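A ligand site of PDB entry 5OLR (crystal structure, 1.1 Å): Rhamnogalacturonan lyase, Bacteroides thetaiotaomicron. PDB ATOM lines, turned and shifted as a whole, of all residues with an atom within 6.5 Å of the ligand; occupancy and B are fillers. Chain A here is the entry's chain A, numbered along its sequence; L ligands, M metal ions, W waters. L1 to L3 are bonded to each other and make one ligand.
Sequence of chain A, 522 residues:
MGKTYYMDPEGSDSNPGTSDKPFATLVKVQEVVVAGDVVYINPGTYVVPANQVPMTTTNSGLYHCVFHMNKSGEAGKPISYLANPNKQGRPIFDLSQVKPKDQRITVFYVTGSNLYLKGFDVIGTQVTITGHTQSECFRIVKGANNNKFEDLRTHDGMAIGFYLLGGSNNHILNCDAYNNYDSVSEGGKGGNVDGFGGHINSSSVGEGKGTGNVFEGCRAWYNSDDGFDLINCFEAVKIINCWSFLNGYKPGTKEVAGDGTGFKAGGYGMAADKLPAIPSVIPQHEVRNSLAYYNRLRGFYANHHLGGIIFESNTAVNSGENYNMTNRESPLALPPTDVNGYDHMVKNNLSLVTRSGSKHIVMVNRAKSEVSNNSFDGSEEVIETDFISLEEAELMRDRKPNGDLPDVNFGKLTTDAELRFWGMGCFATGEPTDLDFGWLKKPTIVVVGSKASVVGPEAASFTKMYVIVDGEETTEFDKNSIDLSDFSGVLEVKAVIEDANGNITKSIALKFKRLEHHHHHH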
ATOM      1  N   ASN A  59     -30.282 -12.495  -8.621  1.00  0.00           N
ATOM      2  CA  ASN A  59     -29.138 -11.851  -9.273  1.00  0.00           C
ATOM      3  C   ASN A  59     -29.314 -10.328  -9.300  1.00  0.00           C
ATOM      4  O   ASN A  59     -29.299  -9.678 -10.357  1.00  0.00           O
ATOM      5  CB  ASN A  59     -28.922 -12.454 -10.675  1.00  0.00           C
ATOM      6  CG  ASN A  59     -28.523 -13.904 -10.636  1.00  0.00           C
ATOM      7  OD1 ASN A  59     -29.377 -14.793 -10.727  1.00  0.00           O
ATOM      8  ND2 ASN A  59     -27.256 -14.160 -10.440  1.00  0.00           N
ATOM      9  N   LEU A  62     -32.000  -9.040 -11.664  1.00  0.00           N
ATOM     10  CA  LEU A  62     -31.931  -9.377 -13.073  1.00  0.00           C
ATOM     11  C   LEU A  62     -33.061 -10.317 -13.467  1.00  0.00           C
ATOM     12  O   LEU A  62     -33.591 -10.208 -14.591  1.00  0.00           O
ATOM     13  CB  LEU A  62     -30.582 -10.033 -13.372  1.00  0.00           C
ATOM     14  CG  LEU A  62     -30.357 -10.523 -14.786  1.00  0.00           C
ATOM     15  CD1 LEU A  62     -30.447  -9.381 -15.797  1.00  0.00           C
ATOM     16  CD2 LEU A  62     -29.038 -11.288 -14.888  1.00  0.00           C
ATOM     17  N   TYR A  63     -33.381 -11.285 -12.594  1.00  0.00           N
ATOM     18  CA  TYR A  63     -34.407 -12.270 -12.909  1.00  0.00           C
ATOM     19  C   TYR A  63     -35.740 -11.970 -12.232  1.00  0.00           C
ATOM     20  O   TYR A  63     -35.805 -11.737 -11.028  1.00  0.00           O
ATOM     21  CB  TYR A  63     -33.984 -13.659 -12.454  1.00  0.00           C
ATOM     22  CG  TYR A  63     -33.074 -14.385 -13.436  1.00  0.00           C
ATOM     23  CD1 TYR A  63     -33.602 -15.120 -14.443  1.00  0.00           C
ATOM     24  CD2 TYR A  63     -31.689 -14.371 -13.282  1.00  0.00           C
ATOM     25  CE1 TYR A  63     -32.806 -15.825 -15.325  1.00  0.00           C
ATOM     26  CE2 TYR A  63     -30.876 -15.090 -14.129  1.00  0.00           C
ATOM     27  CZ  TYR A  63     -31.422 -15.823 -15.143  1.00  0.00           C
ATOM     28  OH  TYR A  63     -30.607 -16.545 -15.999  1.00  0.00           O
ATOM     29  N   ARG A 104     -34.619 -10.873 -17.130  1.00  0.00           N
ATOM     30  CA  ARG A 104     -34.704 -12.254 -17.565  1.00  0.00           C
ATOM     31  C   ARG A 104     -35.876 -12.922 -16.878  1.00  0.00           C
ATOM     32  O   ARG A 104     -36.293 -12.475 -15.809  1.00  0.00           O
ATOM     33  CB  ARG A 104     -33.433 -12.995 -17.189  1.00  0.00           C
ATOM     34  CG  ARG A 104     -32.158 -12.491 -17.860  1.00  0.00           C
ATOM     35  CD  ARG A 104     -30.989 -13.365 -17.440  1.00  0.00           C
ATOM     36  NE  ARG A 104     -29.727 -12.947 -18.055  1.00  0.00           N
ATOM     37  CZ  ARG A 104     -28.597 -13.637 -17.957  1.00  0.00           C
ATOM     38  NH1 ARG A 104     -28.578 -14.819 -17.377  1.00  0.00           N
ATOM     39  NH2 ARG A 104     -27.483 -13.123 -18.471  1.00  0.00           N
ATOM     40  N   HIS A 132     -26.755  -9.776 -24.476  1.00  0.00           N
ATOM     41  CA  HIS A 132     -26.562 -11.131 -23.978  1.00  0.00           C
ATOM     42  C   HIS A 132     -27.577 -11.456 -22.894  1.00  0.00           C
ATOM     43  O   HIS A 132     -27.654 -10.775 -21.890  1.00  0.00           O
ATOM     44  CB  HIS A 132     -25.153 -11.285 -23.399  1.00  0.00           C
ATOM     45  CG  HIS A 132     -24.956 -12.552 -22.640  1.00  0.00           C
ATOM     46  ND1 HIS A 132     -24.766 -13.768 -23.269  1.00  0.00           N
ATOM     47  CD2 HIS A 132     -24.940 -12.814 -21.318  1.00  0.00           C
ATOM     48  CE1 HIS A 132     -24.666 -14.728 -22.357  1.00  0.00           C
ATOM     49  NE2 HIS A 132     -24.748 -14.167 -21.165  1.00  0.00           N
ATOM     50  N   THR A 133     -28.334 -12.531 -23.100  1.00  0.00           N
ATOM     51  CA  THR A 133     -29.413 -12.837 -22.173  1.00  0.00           C
ATOM     52  C   THR A 133     -29.904 -14.266 -22.372  1.00  0.00           C
ATOM     53  O   THR A 133     -29.611 -14.927 -23.367  1.00  0.00           O
ATOM     54  CB  THR A 133     -30.584 -11.830 -22.332  1.00  0.00           C
ATOM     55  OG1 THR A 133     -31.408 -11.838 -21.160  1.00  0.00           O
ATOM     56  CG2 THR A 133     -31.388 -12.090 -23.573  1.00  0.00           C
ATOM     57  N   GLN A 134     -30.765 -14.667 -21.454  1.00  0.00           N
ATOM     58  CA  GLN A 134     -31.510 -15.931 -21.561  1.00  0.00           C
ATOM     59  C   GLN A 134     -32.661 -15.897 -20.590  1.00  0.00           C
ATOM     60  O   GLN A 134     -32.688 -15.093 -19.667  1.00  0.00           O
ATOM     61  CB  GLN A 134     -30.625 -17.146 -21.250  1.00  0.00           C
ATOM     62  CG  GLN A 134     -30.096 -17.112 -19.834  1.00  0.00           C
ATOM     63  CD  GLN A 134     -29.024 -18.144 -19.573  1.00  0.00           C
ATOM     64  OE1 GLN A 134     -28.043 -18.200 -20.296  1.00  0.00           O
ATOM     65  NE2 GLN A 134     -29.267 -18.983 -18.581  1.00  0.00           N
ATOM     66  N   GLU A 136     -35.292 -19.110 -18.646  1.00  0.00           N
ATOM     67  CA  GLU A 136     -35.374 -20.569 -18.415  1.00  0.00           C
ATOM     68  C   GLU A 136     -36.765 -20.959 -17.983  1.00  0.00           C
ATOM     69  O   GLU A 136     -37.371 -20.277 -17.174  1.00  0.00           O
ATOM     70  CB  GLU A 136     -34.380 -21.043 -17.349  1.00  0.00           C
ATOM     71  CG  GLU A 136     -32.968 -20.487 -17.536  1.00  0.00           C
ATOM     72  CD  GLU A 136     -32.686 -19.223 -16.742  1.00  0.00           C
ATOM     73  OE1 GLU A 136     -33.382 -18.955 -15.715  1.00  0.00           O
ATOM     74  OE2 GLU A 136     -31.741 -18.494 -17.145  1.00  0.00           O
ATOM     75  N   ILE A 160     -34.556 -21.533 -22.496  1.00  0.00           N
ATOM     76  CA  ILE A 160     -33.945 -22.808 -22.197  1.00  0.00           C
ATOM     77  C   ILE A 160     -34.959 -23.664 -21.454  1.00  0.00           C
ATOM     78  O   ILE A 160     -35.714 -23.143 -20.627  1.00  0.00           O
ATOM     79  CB  ILE A 160     -32.706 -22.573 -21.287  1.00  0.00           C
ATOM     80  CG1 ILE A 160     -31.654 -21.689 -21.983  1.00  0.00           C
ATOM     81  CG2 ILE A 160     -32.113 -23.861 -20.816  1.00  0.00           C
ATOM     82  CD1 ILE A 160     -30.791 -20.916 -21.013  1.00  0.00           C
ATOM     83  N   TYR A 163     -32.292 -25.865 -16.798  1.00  0.00           N
ATOM     84  CA  TYR A 163     -30.991 -25.236 -16.633  1.00  0.00           C
ATOM     85  C   TYR A 163     -30.544 -25.435 -15.200  1.00  0.00           C
ATOM     86  O   TYR A 163     -31.093 -24.820 -14.285  1.00  0.00           O
ATOM     87  CB  TYR A 163     -31.118 -23.759 -17.012  1.00  0.00           C
ATOM     88  CG  TYR A 163     -29.851 -22.963 -17.058  1.00  0.00           C
ATOM     89  CD1 TYR A 163     -29.018 -23.000 -18.161  1.00  0.00           C
ATOM     90  CD2 TYR A 163     -29.525 -22.071 -16.040  1.00  0.00           C
ATOM     91  CE1 TYR A 163     -27.887 -22.214 -18.249  1.00  0.00           C
ATOM     92  CE2 TYR A 163     -28.382 -21.280 -16.104  1.00  0.00           C
ATOM     93  CZ  TYR A 163     -27.561 -21.372 -17.221  1.00  0.00           C
ATOM     94  OH  TYR A 163     -26.431 -20.597 -17.339  1.00  0.00           O
ATOM     95  N   LEU A 165     -27.810 -25.013 -12.364  1.00  0.00           N
ATOM     96  CA  LEU A 165     -26.619 -24.338 -11.833  1.00  0.00           C
ATOM     97  C   LEU A 165     -26.108 -24.961 -10.536  1.00  0.00           C
ATOM     98  O   LEU A 165     -25.018 -24.624 -10.054  1.00  0.00           O
ATOM     99  CB  LEU A 165     -26.882 -22.873 -11.557  1.00  0.00           C
ATOM    100  CG  LEU A 165     -27.111 -22.013 -12.801  1.00  0.00           C
ATOM    101  CD1 LEU A 165     -27.388 -20.591 -12.373  1.00  0.00           C
ATOM    102  CD2 LEU A 165     -25.897 -22.046 -13.716  1.00  0.00           C
ATOM    103  N   GLY A 191     -28.317 -18.263 -29.889  1.00  0.00           N
ATOM    104  CA  GLY A 191     -27.176 -19.022 -29.414  1.00  0.00           C
ATOM    105  C   GLY A 191     -27.128 -19.378 -27.959  1.00  0.00           C
ATOM    106  O   GLY A 191     -26.160 -20.028 -27.557  1.00  0.00           O
ATOM    107  N   ASN A 192     -28.130 -19.008 -27.163  1.00  0.00           N
ATOM    108  CA  ASN A 192     -28.142 -19.398 -25.760  1.00  0.00           C
ATOM    109  C   ASN A 192     -29.300 -20.302 -25.401  1.00  0.00           C
ATOM    110  O   ASN A 192     -29.466 -20.611 -24.236  1.00  0.00           O
ATOM    111  CB  ASN A 192     -28.136 -18.162 -24.855  1.00  0.00           C
ATOM    112  CG  ASN A 192     -26.919 -17.292 -25.076  1.00  0.00           C
ATOM    113  OD1 ASN A 192     -25.814 -17.786 -25.256  1.00  0.00           O
ATOM    114  ND2 ASN A 192     -27.130 -16.005 -25.150  1.00  0.00           N
ATOM    115  N   ASP A 194     -30.728 -23.782 -25.225  1.00  0.00           N
ATOM    116  CA  ASP A 194     -30.567 -25.204 -25.235  1.00  0.00           C
ATOM    117  C   ASP A 194     -31.852 -25.860 -24.696  1.00  0.00           C
ATOM    118  O   ASP A 194     -32.573 -25.245 -23.921  1.00  0.00           O
ATOM    119  CB  ASP A 194     -29.395 -25.627 -24.324  1.00  0.00           C
ATOM    120  CG  ASP A 194     -28.036 -25.136 -24.776  1.00  0.00           C
ATOM    121  OD1 ASP A 194     -27.839 -24.945 -26.005  1.00  0.00           O
ATOM    122  OD2 ASP A 194     -27.141 -25.007 -23.938  1.00  0.00           O
ATOM    123  N   GLY A 197     -29.608 -28.019 -19.999  1.00  0.00           N
ATOM    124  CA  GLY A 197     -28.300 -27.504 -19.621  1.00  0.00           C
ATOM    125  C   GLY A 197     -27.895 -27.976 -18.256  1.00  0.00           C
ATOM    126  O   GLY A 197     -28.616 -27.770 -17.268  1.00  0.00           O
ATOM    127  N   HIS A 199     -24.919 -27.324 -15.699  1.00  0.00           N
ATOM    128  CA  HIS A 199     -23.841 -26.332 -15.483  1.00  0.00           C
ATOM    129  C   HIS A 199     -23.646 -26.101 -13.982  1.00  0.00           C
ATOM    130  O   HIS A 199     -23.647 -24.976 -13.501  1.00  0.00           O
ATOM    131  CB  HIS A 199     -24.151 -25.013 -16.213  1.00  0.00           C
ATOM    132  CG  HIS A 199     -24.682 -25.174 -17.586  1.00  0.00           C
ATOM    133  ND1 HIS A 199     -23.917 -25.631 -18.632  1.00  0.00           N
ATOM    134  CD2 HIS A 199     -25.905 -24.895 -18.097  1.00  0.00           C
ATOM    135  CE1 HIS A 199     -24.658 -25.629 -19.726  1.00  0.00           C
ATOM    136  NE2 HIS A 199     -25.870 -25.188 -19.434  1.00  0.00           N
ATOM    137  N   ASP A 225     -29.902 -23.499 -30.122  1.00  0.00           N
ATOM    138  CA  ASP A 225     -28.500 -23.729 -29.902  1.00  0.00           C
ATOM    139  C   ASP A 225     -28.223 -25.222 -29.898  1.00  0.00           C
ATOM    140  O   ASP A 225     -28.070 -25.820 -30.981  1.00  0.00           O
ATOM    141  CB  ASP A 225     -27.997 -22.937 -28.654  1.00  0.00           C
ATOM    142  CG  ASP A 225     -26.512 -22.735 -28.604  1.00  0.00           C
ATOM    143  OD1 ASP A 225     -25.943 -22.273 -29.639  1.00  0.00           O
ATOM    144  OD2 ASP A 225     -25.887 -22.952 -27.560  1.00  0.00           O
ATOM    145  N   ASP A 229     -26.358 -29.597 -23.174  1.00  0.00           N
ATOM    146  CA  ASP A 229     -25.096 -28.860 -23.013  1.00  0.00           C
ATOM    147  C   ASP A 229     -24.649 -28.934 -21.566  1.00  0.00           C
ATOM    148  O   ASP A 229     -25.391 -28.512 -20.668  1.00  0.00           O
ATOM    149  CB  ASP A 229     -25.338 -27.430 -23.526  1.00  0.00           C
ATOM    150  CG  ASP A 229     -24.156 -26.497 -23.398  1.00  0.00           C
ATOM    151  OD1 ASP A 229     -23.333 -26.643 -22.499  1.00  0.00           O
ATOM    152  OD2 ASP A 229     -24.132 -25.515 -24.207  1.00  0.00           O
ATOM    153  N   ILE A 231     -21.484 -27.610 -20.566  1.00  0.00           N
ATOM    154  CA  ILE A 231     -20.313 -26.743 -20.354  1.00  0.00           C
ATOM    155  C   ILE A 231     -20.282 -26.216 -18.914  1.00  0.00           C
ATOM    156  O   ILE A 231     -21.292 -26.035 -18.267  1.00  0.00           O
ATOM    157  CB  ILE A 231     -20.306 -25.555 -21.374  1.00  0.00           C
ATOM    158  CG1 ILE A 231     -18.890 -25.040 -21.612  1.00  0.00           C
ATOM    159  CG2 ILE A 231     -21.267 -24.458 -20.973  1.00  0.00           C
ATOM    160  CD1 ILE A 231     -18.803 -23.953 -22.674  1.00  0.00           C
ATOM    161  N   ASN A 232     -19.084 -25.938 -18.425  1.00  0.00           N
ATOM    162  CA  ASN A 232     -18.911 -25.293 -17.135  1.00  0.00           C
ATOM    163  C   ASN A 232     -19.655 -26.033 -16.028  1.00  0.00           C
ATOM    164  O   ASN A 232     -20.326 -25.421 -15.189  1.00  0.00           O
ATOM    165  CB  ASN A 232     -19.268 -23.816 -17.217  1.00  0.00           C
ATOM    166  CG  ASN A 232     -18.322 -23.063 -18.122  1.00  0.00           C
ATOM    167  OD1 ASN A 232     -17.109 -23.256 -18.040  1.00  0.00           O
ATOM    168  ND2 ASN A 232     -18.851 -22.194 -18.971  1.00  0.00           N
HETATM  169  C1  LIG L   1     -22.362 -19.683 -21.926  1.00  0.00           C
HETATM  170  C2  LIG L   1     -23.079 -18.497 -21.295  1.00  0.00           C
HETATM  171  C3  LIG L   1     -24.603 -18.675 -21.402  1.00  0.00           C
HETATM  172  C4  LIG L   1     -25.013 -19.996 -20.773  1.00  0.00           C
HETATM  173  C5  LIG L   1     -24.256 -21.123 -21.485  1.00  0.00           C
HETATM  174  C6  LIG L   1     -24.534 -22.495 -20.902  1.00  0.00           C
HETATM  175  O1  LIG L   1     -22.557 -19.682 -23.322  1.00  0.00           O
HETATM  176  O2  LIG L   1     -22.707 -18.530 -19.915  1.00  0.00           O
HETATM  177  O3  LIG L   1     -25.248 -17.542 -20.804  1.00  0.00           O
HETATM  178  O4  LIG L   1     -26.408 -20.208 -20.970  1.00  0.00           O
HETATM  179  O5  LIG L   1     -22.860 -20.897 -21.340  1.00  0.00           O
HETATM  180  C1  LG2 L   2     -22.135 -17.363 -19.333  1.00  0.00           C
HETATM  181  C2  LG2 L   2     -21.343 -17.779 -18.098  1.00  0.00           C
HETATM  182  C3  LG2 L   2     -22.279 -18.232 -17.011  1.00  0.00           C
HETATM  183  C4  LG2 L   2     -23.347 -17.180 -16.765  1.00  0.00           C
HETATM  184  C5  LG2 L   2     -24.084 -16.867 -18.062  1.00  0.00           C
HETATM  185  C6  LG2 L   2     -25.187 -15.869 -17.907  1.00  0.00           C
HETATM  186  O1  LG2 L   2     -20.454 -18.849 -18.445  1.00  0.00           O
HETATM  187  O2  LG2 L   2     -21.533 -18.524 -15.835  1.00  0.00           O
HETATM  188  O3  LG2 L   2     -22.778 -15.966 -16.239  1.00  0.00           O
HETATM  189  O4  LG2 L   2     -23.135 -16.377 -19.034  1.00  0.00           O
HETATM  190  O5  LG2 L   2     -26.151 -16.218 -17.173  1.00  0.00           O
HETATM  191  O6  LG2 L   2     -25.129 -14.763 -18.518  1.00  0.00           O
HETATM  192  C1  LG3 L   3     -22.806 -15.852 -14.844  1.00  0.00           C
HETATM  193  C2  LG3 L   3     -21.784 -14.845 -14.403  1.00  0.00           C
HETATM  194  C3  LG3 L   3     -22.299 -13.474 -14.825  1.00  0.00           C
HETATM  195  C4  LG3 L   3     -23.732 -13.240 -14.325  1.00  0.00           C
HETATM  196  C5  LG3 L   3     -24.666 -14.375 -14.783  1.00  0.00           C
HETATM  197  C6  LG3 L   3     -26.067 -14.256 -14.210  1.00  0.00           C
HETATM  198  O1  LG3 L   3     -21.673 -14.913 -12.983  1.00  0.00           O
HETATM  199  O2  LG3 L   3     -21.444 -12.441 -14.315  1.00  0.00           O
HETATM  200  O3  LG3 L   3     -24.229 -12.027 -14.844  1.00  0.00           O
HETATM  201  O4  LG3 L   3     -24.100 -15.606 -14.359  1.00  0.00           O
HETATM  202 CA    CA M   1     -24.182 -21.348 -27.669  1.00  0.00          CA
HETATM  203 CA    CA M   2     -25.453 -24.275 -25.688  1.00  0.00          CA
HETATM  204  O   HOH W   1     -25.473 -10.731 -12.715  1.00  0.00           O
HETATM  205  O   HOH W   2     -19.670 -17.804 -23.575  1.00  0.00           O
HETATM  206  O   HOH W   3     -21.655 -21.322 -18.847  1.00  0.00           O
HETATM  207  O   HOH W   4     -23.558 -15.199 -10.948  1.00  0.00           O
HETATM  208  O   HOH W   5     -22.299 -13.606 -18.786  1.00  0.00           O
HETATM  209  O   HOH W   6     -18.855 -18.188 -20.697  1.00  0.00           O
HETATM  210  O   HOH W   7     -26.487 -18.527 -15.766  1.00  0.00           O
HETATM  211  O   HOH W   8     -27.836 -21.952 -22.422  1.00  0.00           O
HETATM  212  O   HOH W   9     -25.067 -17.975 -13.374  1.00  0.00           O
HETATM  213  O   HOH W  10     -23.932 -11.333 -17.494  1.00  0.00           O
HETATM  214  O   HOH W  11     -22.489 -21.014 -14.782  1.00  0.00           O
HETATM  215  O   HOH W  12     -23.269 -16.911 -24.435  1.00  0.00           O
HETATM  216  O   HOH W  13     -20.006 -16.791 -12.135  1.00  0.00           O
HETATM  217  O   HOH W  14     -24.564 -20.156 -25.288  1.00  0.00           O
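Water W8 lies within hydrogen-bond range of O4 of LIG L1 (2.7 Å) and O of Asn 192 (2.8 Å).
Water W7 bridges OH of Tyr 163 and O5 of LG2 L2.
Water W3 bridges an oxygen (O1) of LG2 L2 (2.8 Å) and the side-chain amide nitrogen (ND2) of Asn 232 (2.9 Å).
Water W14 lies within hydrogen-bond range of OD1 of Asn 192 and O1 of LIG L1.
Water W5 bridges O4 of LG2 L2 (2.9 Å) and NE2 of His 132 (3.5 Å).
Water W12 bridges OD1 of Asn 192 (2.8 Å) and O1 of LIG L1 (3.1 Å).
The side-chain amide oxygen of Gln 134 is in hydrogen-bond range of an oxygen (O4) of LIG L1, 2.7 Å away.
A ring nitrogen (NE2) of His 132 lies within hydrogen-bond range of an oxygen (O6) of LG2 L2, 2.7 Å away.
The guanidinium group (NH1) of Arg 104 is in salt-bridge range of an oxygen (O5) of LG2 L2, 2.8 Å away.
Merely in contact with the ligand: His 199 (3.3 Å), Tyr 163 (3.7 Å), Asn 232 (3.7 Å), Ile 231 (3.8 Å) and Asn 59 (3.95 Å).
Hydrophobic or aromatic side chains that line the ligand: His 132, Tyr 163, His 199 and Ile 231.
The nearest printed residue that does not touch the ligand is Asn 192 (4.1 Å).
The side-chain amide nitrogen of Gln 134 sits close to the side-chain hydroxyl of Tyr 163 (3.5 Å).
The side-chain amide nitrogen (NE2) of Gln 134 is in hydrogen-bond range of the side-chain carboxylate (OE2) of Glu 136 (2.9 Å).
The backbone carbonyl oxygen of Leu 62 is in hydrogen-bond range of the backbone NH of Arg 104 (2.8 Å).
NH1 of Arg 104 sits at hydrogen-bond distance from OH of Tyr 63 (3.0 Å).
ND1 of His 199 lies within hydrogen-bond range of O of Ile 231 (2.7 Å).
OD1 of Asp 229 lies within hydrogen-bond range of N of Ile 231, 2.8 Å away.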
